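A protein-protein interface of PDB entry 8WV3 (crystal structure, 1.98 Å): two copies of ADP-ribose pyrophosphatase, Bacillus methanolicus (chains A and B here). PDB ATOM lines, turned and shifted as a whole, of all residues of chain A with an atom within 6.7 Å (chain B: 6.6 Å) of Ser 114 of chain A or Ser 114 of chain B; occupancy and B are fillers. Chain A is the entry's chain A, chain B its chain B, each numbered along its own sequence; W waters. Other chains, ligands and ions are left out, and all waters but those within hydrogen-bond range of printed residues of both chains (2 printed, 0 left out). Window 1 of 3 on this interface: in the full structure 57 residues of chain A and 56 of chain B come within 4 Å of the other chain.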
ATOM      1  N   PRO A  67      23.854 -26.773  13.671  1.00  0.00           N
ATOM      2  CA  PRO A  67      22.722 -25.834  13.546  1.00  0.00           C
ATOM      3  C   PRO A  67      21.390 -26.452  13.934  1.00  0.00           C
ATOM      4  O   PRO A  67      20.533 -25.752  14.481  1.00  0.00           O
ATOM      5  CB  PRO A  67      22.767 -25.428  12.065  1.00  0.00           C
ATOM      6  CG  PRO A  67      24.203 -25.614  11.663  1.00  0.00           C
ATOM      7  CD  PRO A  67      24.620 -26.880  12.417  1.00  0.00           C
ATOM      8  N   LEU A  68      21.212 -27.763  13.740  1.00  0.00           N
ATOM      9  CA  LEU A  68      19.967 -28.434  14.100  1.00  0.00           C
ATOM     10  C   LEU A  68      19.958 -28.974  15.520  1.00  0.00           C
ATOM     11  O   LEU A  68      18.896 -29.394  15.984  1.00  0.00           O
ATOM     12  CB  LEU A  68      19.690 -29.616  13.160  1.00  0.00           C
ATOM     13  CG  LEU A  68      19.649 -29.253  11.683  1.00  0.00           C
ATOM     14  CD1 LEU A  68      19.306 -30.430  10.768  1.00  0.00           C
ATOM     15  CD2 LEU A  68      18.621 -28.138  11.546  1.00  0.00           C
ATOM     16  N   ALA A 112      18.944 -24.671  -5.600  1.00  0.00           N
ATOM     17  CA  ALA A 112      19.324 -23.879  -4.435  1.00  0.00           C
ATOM     18  C   ALA A 112      18.636 -24.440  -3.197  1.00  0.00           C
ATOM     19  O   ALA A 112      17.513 -24.923  -3.259  1.00  0.00           O
ATOM     20  CB  ALA A 112      18.922 -22.407  -4.610  1.00  0.00           C
ATOM     21  N   THR A 113      19.313 -24.362  -2.059  1.00  0.00           N
ATOM     22  CA  THR A 113      18.706 -24.866  -0.831  1.00  0.00           C
ATOM     23  C   THR A 113      17.810 -23.846  -0.135  1.00  0.00           C
ATOM     24  O   THR A 113      16.719 -24.211   0.311  1.00  0.00           O
ATOM     25  CB  THR A 113      19.802 -25.312   0.131  1.00  0.00           C
ATOM     26  OG1 THR A 113      20.790 -24.290   0.171  1.00  0.00           O
ATOM     27  CG2 THR A 113      20.452 -26.570  -0.389  1.00  0.00           C
ATOM     28  N   SER A 114      18.245 -22.577  -0.023  1.00  0.00           N
ATOM     29  CA  SER A 114      17.486 -21.525   0.675  1.00  0.00           C
ATOM     30  C   SER A 114      17.653 -20.228  -0.094  1.00  0.00           C
ATOM     31  O   SER A 114      18.431 -19.350   0.294  1.00  0.00           O
ATOM     32  CB  SER A 114      17.974 -21.315   2.109  1.00  0.00           C
ATOM     33  OG  SER A 114      18.387 -22.530   2.704  1.00  0.00           O
ATOM     34  N   PRO A 115      16.949 -20.075  -1.212  1.00  0.00           N
ATOM     35  CA  PRO A 115      17.226 -18.939  -2.093  1.00  0.00           C
ATOM     36  C   PRO A 115      16.818 -17.616  -1.484  1.00  0.00           C
ATOM     37  O   PRO A 115      17.171 -16.561  -2.036  1.00  0.00           O
ATOM     38  CB  PRO A 115      16.412 -19.270  -3.353  1.00  0.00           C
ATOM     39  CG  PRO A 115      15.255 -20.043  -2.835  1.00  0.00           C
ATOM     40  CD  PRO A 115      15.874 -20.928  -1.735  1.00  0.00           C
ATOM     41  N   GLY A 116      16.101 -17.639  -0.358  1.00  0.00           N
ATOM     42  CA  GLY A 116      15.752 -16.413   0.347  1.00  0.00           C
ATOM     43  C   GLY A 116      16.938 -15.674   0.950  1.00  0.00           C
ATOM     44  O   GLY A 116      16.845 -14.466   1.186  1.00  0.00           O
ATOM     45  N   PHE A 117      18.052 -16.361   1.206  1.00  0.00           N
ATOM     46  CA  PHE A 117      19.176 -15.691   1.856  1.00  0.00           C
ATOM     47  C   PHE A 117      20.539 -16.257   1.470  1.00  0.00           C
ATOM     48  O   PHE A 117      21.555 -15.639   1.784  1.00  0.00           O
ATOM     49  CB  PHE A 117      19.002 -15.731   3.382  1.00  0.00           C
ATOM     50  CG  PHE A 117      19.173 -17.110   3.997  1.00  0.00           C
ATOM     51  CD1 PHE A 117      20.422 -17.570   4.369  1.00  0.00           C
ATOM     52  CD2 PHE A 117      18.074 -17.930   4.214  1.00  0.00           C
ATOM     53  CE1 PHE A 117      20.575 -18.847   4.944  1.00  0.00           C
ATOM     54  CE2 PHE A 117      18.223 -19.198   4.791  1.00  0.00           C
ATOM     55  CZ  PHE A 117      19.482 -19.650   5.148  1.00  0.00           C
ATOM     56  N   ALA A 118      20.589 -17.407   0.784  1.00  0.00           N
ATOM     57  CA  ALA A 118      21.851 -18.092   0.496  1.00  0.00           C
ATOM     58  C   ALA A 118      21.979 -18.382  -0.987  1.00  0.00           C
ATOM     59  O   ALA A 118      20.988 -18.666  -1.664  1.00  0.00           O
ATOM     60  CB  ALA A 118      21.963 -19.415   1.267  1.00  0.00           C
ATOM     61  N   ASP A 119      23.204 -18.314  -1.513  1.00  0.00           N
ATOM     62  CA  ASP A 119      23.365 -18.660  -2.916  1.00  0.00           C
ATOM     63  C   ASP A 119      23.776 -20.121  -3.074  1.00  0.00           C
ATOM     64  O   ASP A 119      24.237 -20.513  -4.148  1.00  0.00           O
ATOM     65  CB  ASP A 119      24.405 -17.780  -3.607  1.00  0.00           C
ATOM     66  CG  ASP A 119      25.768 -17.899  -3.000  1.00  0.00           C
ATOM     67  OD1 ASP A 119      26.693 -17.210  -3.497  1.00  0.00           O
ATOM     68  OD2 ASP A 119      25.972 -18.749  -2.122  1.00  0.00           O
ATOM     69  N   GLU A 120      23.641 -20.924  -2.019  1.00  0.00           N
ATOM     70  CA  GLU A 120      24.167 -22.287  -2.054  1.00  0.00           C
ATOM     71  C   GLU A 120      23.393 -23.129  -3.055  1.00  0.00           C
ATOM     72  O   GLU A 120      22.157 -23.167  -3.011  1.00  0.00           O
ATOM     73  CB  GLU A 120      24.052 -22.947  -0.691  1.00  0.00           C
ATOM     74  CG  GLU A 120      24.334 -24.472  -0.807  1.00  0.00           C
ATOM     75  CD  GLU A 120      24.126 -25.229   0.500  1.00  0.00           C
ATOM     76  OE1 GLU A 120      23.259 -24.817   1.282  1.00  0.00           O
ATOM     77  OE2 GLU A 120      24.886 -26.186   0.773  1.00  0.00           O
ATOM     78  N   ASP A 166      16.587 -33.530   5.672  1.00  0.00           N
ATOM     79  CA  ASP A 166      17.125 -32.392   4.936  1.00  0.00           C
ATOM     80  C   ASP A 166      16.758 -32.524   3.464  1.00  0.00           C
ATOM     81  O   ASP A 166      16.400 -33.611   2.983  1.00  0.00           O
ATOM     82  CB  ASP A 166      18.630 -32.223   5.187  1.00  0.00           C
ATOM     83  CG  ASP A 166      19.505 -33.060   4.294  1.00  0.00           C
ATOM     84  OD1 ASP A 166      19.229 -34.259   4.089  1.00  0.00           O
ATOM     85  OD2 ASP A 166      20.506 -32.501   3.804  1.00  0.00           O
ATOM     86  N   SER A 167      16.784 -31.385   2.756  1.00  0.00           N
ATOM     87  CA  SER A 167      16.139 -31.361   1.438  1.00  0.00           C
ATOM     88  C   SER A 167      16.840 -32.293   0.444  1.00  0.00           C
ATOM     89  O   SER A 167      16.177 -32.981  -0.342  1.00  0.00           O
ATOM     90  CB  SER A 167      16.067 -29.929   0.896  1.00  0.00           C
ATOM     91  OG  SER A 167      17.295 -29.247   0.998  1.00  0.00           O
ATOM     92  N   HIS B  43      17.454 -18.787  11.310  1.00  0.00           N
ATOM     93  CA  HIS B  43      16.427 -18.367  10.403  1.00  0.00           C
ATOM     94  C   HIS B  43      15.133 -18.981  10.924  1.00  0.00           C
ATOM     95  O   HIS B  43      15.125 -20.172  11.265  1.00  0.00           O
ATOM     96  CB  HIS B  43      16.725 -18.834   8.972  1.00  0.00           C
ATOM     97  CG  HIS B  43      15.785 -18.291   7.952  1.00  0.00           C
ATOM     98  ND1 HIS B  43      14.451 -18.630   7.921  1.00  0.00           N
ATOM     99  CD2 HIS B  43      15.977 -17.413   6.938  1.00  0.00           C
ATOM    100  CE1 HIS B  43      13.860 -17.984   6.928  1.00  0.00           C
ATOM    101  NE2 HIS B  43      14.762 -17.239   6.318  1.00  0.00           N
ATOM    102  N   PRO B  67      20.002 -13.586  -3.872  1.00  0.00           N
ATOM    103  CA  PRO B  67      21.195 -14.437  -3.717  1.00  0.00           C
ATOM    104  C   PRO B  67      21.554 -15.196  -4.974  1.00  0.00           C
ATOM    105  O   PRO B  67      22.738 -15.437  -5.220  1.00  0.00           O
ATOM    106  CB  PRO B  67      20.807 -15.372  -2.565  1.00  0.00           C
ATOM    107  CG  PRO B  67      19.864 -14.522  -1.719  1.00  0.00           C
ATOM    108  CD  PRO B  67      19.035 -13.781  -2.780  1.00  0.00           C
ATOM    109  N   LEU B  68      20.570 -15.542  -5.796  1.00  0.00           N
ATOM    110  CA  LEU B  68      20.769 -16.343  -6.997  1.00  0.00           C
ATOM    111  C   LEU B  68      20.969 -15.497  -8.249  1.00  0.00           C
ATOM    112  O   LEU B  68      21.359 -16.035  -9.292  1.00  0.00           O
ATOM    113  CB  LEU B  68      19.557 -17.255  -7.215  1.00  0.00           C
ATOM    114  CG  LEU B  68      19.169 -18.208  -6.073  1.00  0.00           C
ATOM    115  CD1 LEU B  68      18.012 -19.093  -6.501  1.00  0.00           C
ATOM    116  CD2 LEU B  68      20.355 -19.027  -5.589  1.00  0.00           C
ATOM    117  N   ALA B 112      15.055 -29.741   7.064  1.00  0.00           N
ATOM    118  CA  ALA B 112      16.028 -28.647   7.040  1.00  0.00           C
ATOM    119  C   ALA B 112      16.506 -28.385   5.622  1.00  0.00           C
ATOM    120  O   ALA B 112      16.709 -29.315   4.837  1.00  0.00           O
ATOM    121  CB  ALA B 112      17.241 -28.975   7.914  1.00  0.00           C
ATOM    122  N   THR B 113      16.686 -27.103   5.273  1.00  0.00           N
ATOM    123  CA  THR B 113      17.127 -26.821   3.906  1.00  0.00           C
ATOM    124  C   THR B 113      18.619 -27.018   3.740  1.00  0.00           C
ATOM    125  O   THR B 113      19.063 -27.555   2.720  1.00  0.00           O
ATOM    126  CB  THR B 113      16.802 -25.395   3.500  1.00  0.00           C
ATOM    127  OG1 THR B 113      17.177 -24.513   4.580  1.00  0.00           O
ATOM    128  CG2 THR B 113      15.324 -25.292   3.167  1.00  0.00           C
ATOM    129  N   SER B 114      19.407 -26.568   4.717  1.00  0.00           N
ATOM    130  CA  SER B 114      20.867 -26.542   4.606  1.00  0.00           C
ATOM    131  C   SER B 114      21.465 -26.814   5.973  1.00  0.00           C
ATOM    132  O   SER B 114      22.025 -25.916   6.605  1.00  0.00           O
ATOM    133  CB  SER B 114      21.354 -25.193   4.078  1.00  0.00           C
ATOM    134  OG  SER B 114      20.442 -24.652   3.128  1.00  0.00           O
ATOM    135  N   PRO B 115      21.374 -28.059   6.460  1.00  0.00           N
ATOM    136  CA  PRO B 115      21.741 -28.333   7.856  1.00  0.00           C
ATOM    137  C   PRO B 115      23.224 -28.170   8.163  1.00  0.00           C
ATOM    138  O   PRO B 115      23.593 -28.210   9.349  1.00  0.00           O
ATOM    139  CB  PRO B 115      21.306 -29.789   8.049  1.00  0.00           C
ATOM    140  CG  PRO B 115      21.415 -30.379   6.686  1.00  0.00           C
ATOM    141  CD  PRO B 115      20.878 -29.275   5.793  1.00  0.00           C
ATOM    142  N   GLY B 116      24.085 -28.008   7.161  1.00  0.00           N
ATOM    143  CA  GLY B 116      25.496 -27.790   7.455  1.00  0.00           C
ATOM    144  C   GLY B 116      25.826 -26.395   7.975  1.00  0.00           C
ATOM    145  O   GLY B 116      26.903 -26.194   8.549  1.00  0.00           O
ATOM    146  N   PHE B 117      24.947 -25.417   7.771  1.00  0.00           N
ATOM    147  CA  PHE B 117      25.227 -24.095   8.342  1.00  0.00           C
ATOM    148  C   PHE B 117      23.991 -23.346   8.828  1.00  0.00           C
ATOM    149  O   PHE B 117      24.157 -22.333   9.515  1.00  0.00           O
ATOM    150  CB  PHE B 117      25.982 -23.221   7.330  1.00  0.00           C
ATOM    151  CG  PHE B 117      25.133 -22.722   6.196  1.00  0.00           C
ATOM    152  CD1 PHE B 117      24.342 -21.598   6.349  1.00  0.00           C
ATOM    153  CD2 PHE B 117      25.122 -23.378   4.981  1.00  0.00           C
ATOM    154  CE1 PHE B 117      23.550 -21.138   5.310  1.00  0.00           C
ATOM    155  CE2 PHE B 117      24.332 -22.918   3.934  1.00  0.00           C
ATOM    156  CZ  PHE B 117      23.551 -21.790   4.103  1.00  0.00           C
ATOM    157  N   ALA B 118      22.771 -23.791   8.527  1.00  0.00           N
ATOM    158  CA  ALA B 118      21.565 -23.048   8.898  1.00  0.00           C
ATOM    159  C   ALA B 118      20.590 -23.920   9.673  1.00  0.00           C
ATOM    160  O   ALA B 118      20.502 -25.127   9.438  1.00  0.00           O
ATOM    161  CB  ALA B 118      20.852 -22.523   7.647  1.00  0.00           C
ATOM    162  N   ASP B 119      19.786 -23.297  10.543  1.00  0.00           N
ATOM    163  CA  ASP B 119      18.764 -24.058  11.257  1.00  0.00           C
ATOM    164  C   ASP B 119      17.373 -23.906  10.647  1.00  0.00           C
ATOM    165  O   ASP B 119      16.381 -24.238  11.300  1.00  0.00           O
ATOM    166  CB  ASP B 119      18.720 -23.676  12.738  1.00  0.00           C
ATOM    167  CG  ASP B 119      18.223 -22.252  12.960  1.00  0.00           C
ATOM    168  OD1 ASP B 119      17.921 -21.552  11.962  1.00  0.00           O
ATOM    169  OD2 ASP B 119      18.108 -21.861  14.132  1.00  0.00           O
ATOM    170  N   GLU B 120      17.287 -23.442   9.405  1.00  0.00           N
ATOM    171  CA  GLU B 120      15.999 -23.217   8.758  1.00  0.00           C
ATOM    172  C   GLU B 120      15.266 -24.525   8.496  1.00  0.00           C
ATOM    173  O   GLU B 120      15.812 -25.414   7.838  1.00  0.00           O
ATOM    174  CB  GLU B 120      16.206 -22.525   7.430  1.00  0.00           C
ATOM    175  CG  GLU B 120      14.930 -22.416   6.654  1.00  0.00           C
ATOM    176  CD  GLU B 120      15.140 -21.754   5.300  1.00  0.00           C
ATOM    177  OE1 GLU B 120      16.155 -22.056   4.650  1.00  0.00           O
ATOM    178  OE2 GLU B 120      14.285 -20.950   4.881  1.00  0.00           O
ATOM    179  N   ASP B 166      14.726 -24.745  -6.454  1.00  0.00           N
ATOM    180  CA  ASP B 166      14.998 -24.708  -5.015  1.00  0.00           C
ATOM    181  C   ASP B 166      14.397 -25.948  -4.363  1.00  0.00           C
ATOM    182  O   ASP B 166      13.508 -26.583  -4.916  1.00  0.00           O
ATOM    183  CB  ASP B 166      14.474 -23.416  -4.338  1.00  0.00           C
ATOM    184  CG  ASP B 166      12.986 -23.455  -4.006  1.00  0.00           C
ATOM    185  OD1 ASP B 166      12.180 -23.782  -4.892  1.00  0.00           O
ATOM    186  OD2 ASP B 166      12.609 -23.069  -2.868  1.00  0.00           O
ATOM    187  N   SER B 167      14.900 -26.308  -3.181  1.00  0.00           N
ATOM    188  CA  SER B 167      14.660 -27.676  -2.727  1.00  0.00           C
ATOM    189  C   SER B 167      13.186 -27.930  -2.463  1.00  0.00           C
ATOM    190  O   SER B 167      12.662 -28.985  -2.845  1.00  0.00           O
ATOM    191  CB  SER B 167      15.515 -27.986  -1.492  1.00  0.00           C
ATOM    192  OG  SER B 167      15.444 -26.933  -0.568  1.00  0.00           O
HETATM  193  O   HOH W   1      13.624 -24.243  -0.652  1.00  0.00           O
HETATM  194  O   HOH W   2      20.060 -30.436   2.040  1.00  0.00           O
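Ser 114 of chain A touches three residues of chain B. Ser 114 of chain B touches three residues of chain A. Printed residues of chain B within 4 Å of Phe 117 of chain A: His 43, Pro 67, Phe 117 and Glu 120. Printed residues of chain B within 4 Å of Pro 67 of chain A: Pro 115 (3.5 Å), Phe 117 (3.6 Å), Ala 118 (3.5 Å) and Asp 119 (3.3 Å). Of the printed residues of chain B, Glu 120 of chain A touches Ser 114 and Phe 117. Gly 116 of chain A touches none of the printed residues of chain B. Gly 116 of chain B touches none of the printed residues of chain A. The nearest residue of chain B that does not touch Ser 114 of chain A is Ser 167 of chain B (5.2 Å). The nearest residue of chain A that does not touch Ser 114 of chain B is Ser 167 of chain A (5.0 Å).
Among the printed residues, pairs that only touch across the chains: Pro 67 of chain A with Pro 115 of chain B (3.5 Å), Pro 67 of chain A with Phe 117 of chain B (3.6 Å), Pro 67 of chain A with Ala 118 of chain B (3.5 Å), Pro 67 of chain A with Asp 119 of chain B (3.3 Å), Leu 68 of chain A with Ala 112 of chain B (3.8 Å), Leu 68 of chain A with Pro 115 of chain B (3.4 Å), Ala 112 of chain A with Leu 68 of chain B (3.8 Å), Ala 112 of chain A with Asp 166 of chain B (3.1 Å), Thr 113 of chain A with Thr 113 of chain B (3.4 Å), Pro 115 of chain A with Pro 67 of chain B (3.4 Å), Pro 115 of chain A with Leu 68 of chain B (3.5 Å), Pro 115 of chain A with Asp 166 of chain B (3.8 Å), Phe 117 of chain A with His 43 of chain B (3.5 Å), Phe 117 of chain A with Pro 67 of chain B (3.7 Å), Phe 117 of chain A with Phe 117 of chain B (3.8 Å), Phe 117 of chain A with Glu 120 of chain B (3.5 Å), Ala 118 of chain A with Pro 67 of chain B (3.4 Å), Ala 118 of chain A with Leu 68 of chain B (3.99 Å), Asp 119 of chain A with Pro 67 of chain B (3.3 Å), Glu 120 of chain A with Phe 117 of chain B (3.4 Å), Asp 166 of chain A with Ala 112 of chain B (3.1 Å) and Asp 166 of chain A with Pro 115 of chain B (3.7 Å).
Hydrophobic or aromatic side chains of chain A within 4 Å of the printed part of chain B: Pro 67, Leu 68, Ala 112, Pro 115 and Phe 117. Hydrophobic or aromatic side chains of chain B within 4 Å of the printed part of chain A: His 43, Pro 67, Leu 68, Ala 112, Pro 115 and Phe 117. Among the printed residues, no Asp or Glu carboxylate lies within 4 Å of a Lys or Arg side-chain nitrogen of the other chain.
Pro 67 of chain A touches Ala 118 of chain B, and with the chains exchanged Ala 118 of chain A touches Pro 67 of chain B. Thr 113 of chain A touches Ser 114 of chain B, and with the chains exchanged Ser 114 of chain A touches Thr 113 of chain B. Thr 113 of chain A touches Ser 167 of chain B, and with the chains exchanged Ser 167 of chain A touches Thr 113 of chain B. Phe 117 of chain A touches Glu 120 of chain B, and with the chains exchanged Glu 120 of chain A touches Phe 117 of chain B. Positions printed for both chains: 67, 68, 112, 113, 114, 115, 116, 117, 118, 119, 120, 166 and 167. Of the 32 pairs that touch across the chains among the printed residues, 30 have their exchanged pair printed and touching as well.
The backbone NH (N) of His 43 of chain B sits at hydrogen-bond distance from the side-chain carboxylate (OD1) of Asp 119 of chain B (2.9 Å). The side-chain carboxylate (OE1) of Glu 120 of chain A is in hydrogen-bond range of the side-chain hydroxyl (OG1) of Thr 113 of chain A (2.8 Å). OG1 of Thr 113 of chain B is in hydrogen-bond range of OE1 of Glu 120 of chain B (2.7 Å).
Water W1 lies within hydrogen-bond range of the side-chain carboxylate of Asp 166 of chain B (2.7 Å), the backbone carbonyl oxygen of Thr 113 of chain A (3.2 Å) and the side-chain hydroxyl of Ser 167 of chain B (3.2 Å). Water W2 lies within hydrogen-bond range of OD2 of Asp 166 of chain A, O of Thr 113 of chain B and OG of Ser 167 of chain A.
The backbone carbonyl oxygen (O) of Ala 112 of chain A is in hydrogen-bond range of the backbone NH (N) of Ser 167 of chain B (3.0 Å). The side-chain hydroxyl (OG) of Ser 167 of chain B is in hydrogen-bond range of the backbone carbonyl oxygen (O) of Thr 113 of chain A (3.1 Å). The side-chain hydroxyl (OG) of Ser 114 of chain A lies within hydrogen-bond range of the side-chain carboxylate (OE1) of Glu 120 of chain B, 3.0 Å away. The side-chain hydroxyl (OG) of Ser 114 of chain A lies within hydrogen-bond range of the side-chain hydroxyl (OG1) of Thr 113 of chain B, at 3.0 Å. The side-chain hydroxyl (OG1) of Thr 113 of chain A is in hydrogen-bond range of the side-chain hydroxyl (OG) of Ser 114 of chain B, 3.0 Å away. The side-chain hydroxyl (OG) of Ser 114 of chain B sits at hydrogen-bond distance from the side-chain hydroxyl (OG) of Ser 114 of chain A (3.0 Å). The side-chain carboxylate (OE1) of Glu 120 of chain A lies within hydrogen-bond range of the side-chain hydroxyl (OG) of Ser 114 of chain B, at 3.4 Å. OG of Ser 167 of chain A lies within hydrogen-bond range of O of Thr 113 of chain B, at 3.0 Å. The side-chain hydroxyl (OG) of Ser 167 of chain B sits close to the side-chain hydroxyl (OG) of Ser 167 of chain A. The backbone NH of Ser 167 of chain A is in hydrogen-bond range of the backbone carbonyl oxygen of Ala 112 of chain B, at 2.9 Å.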
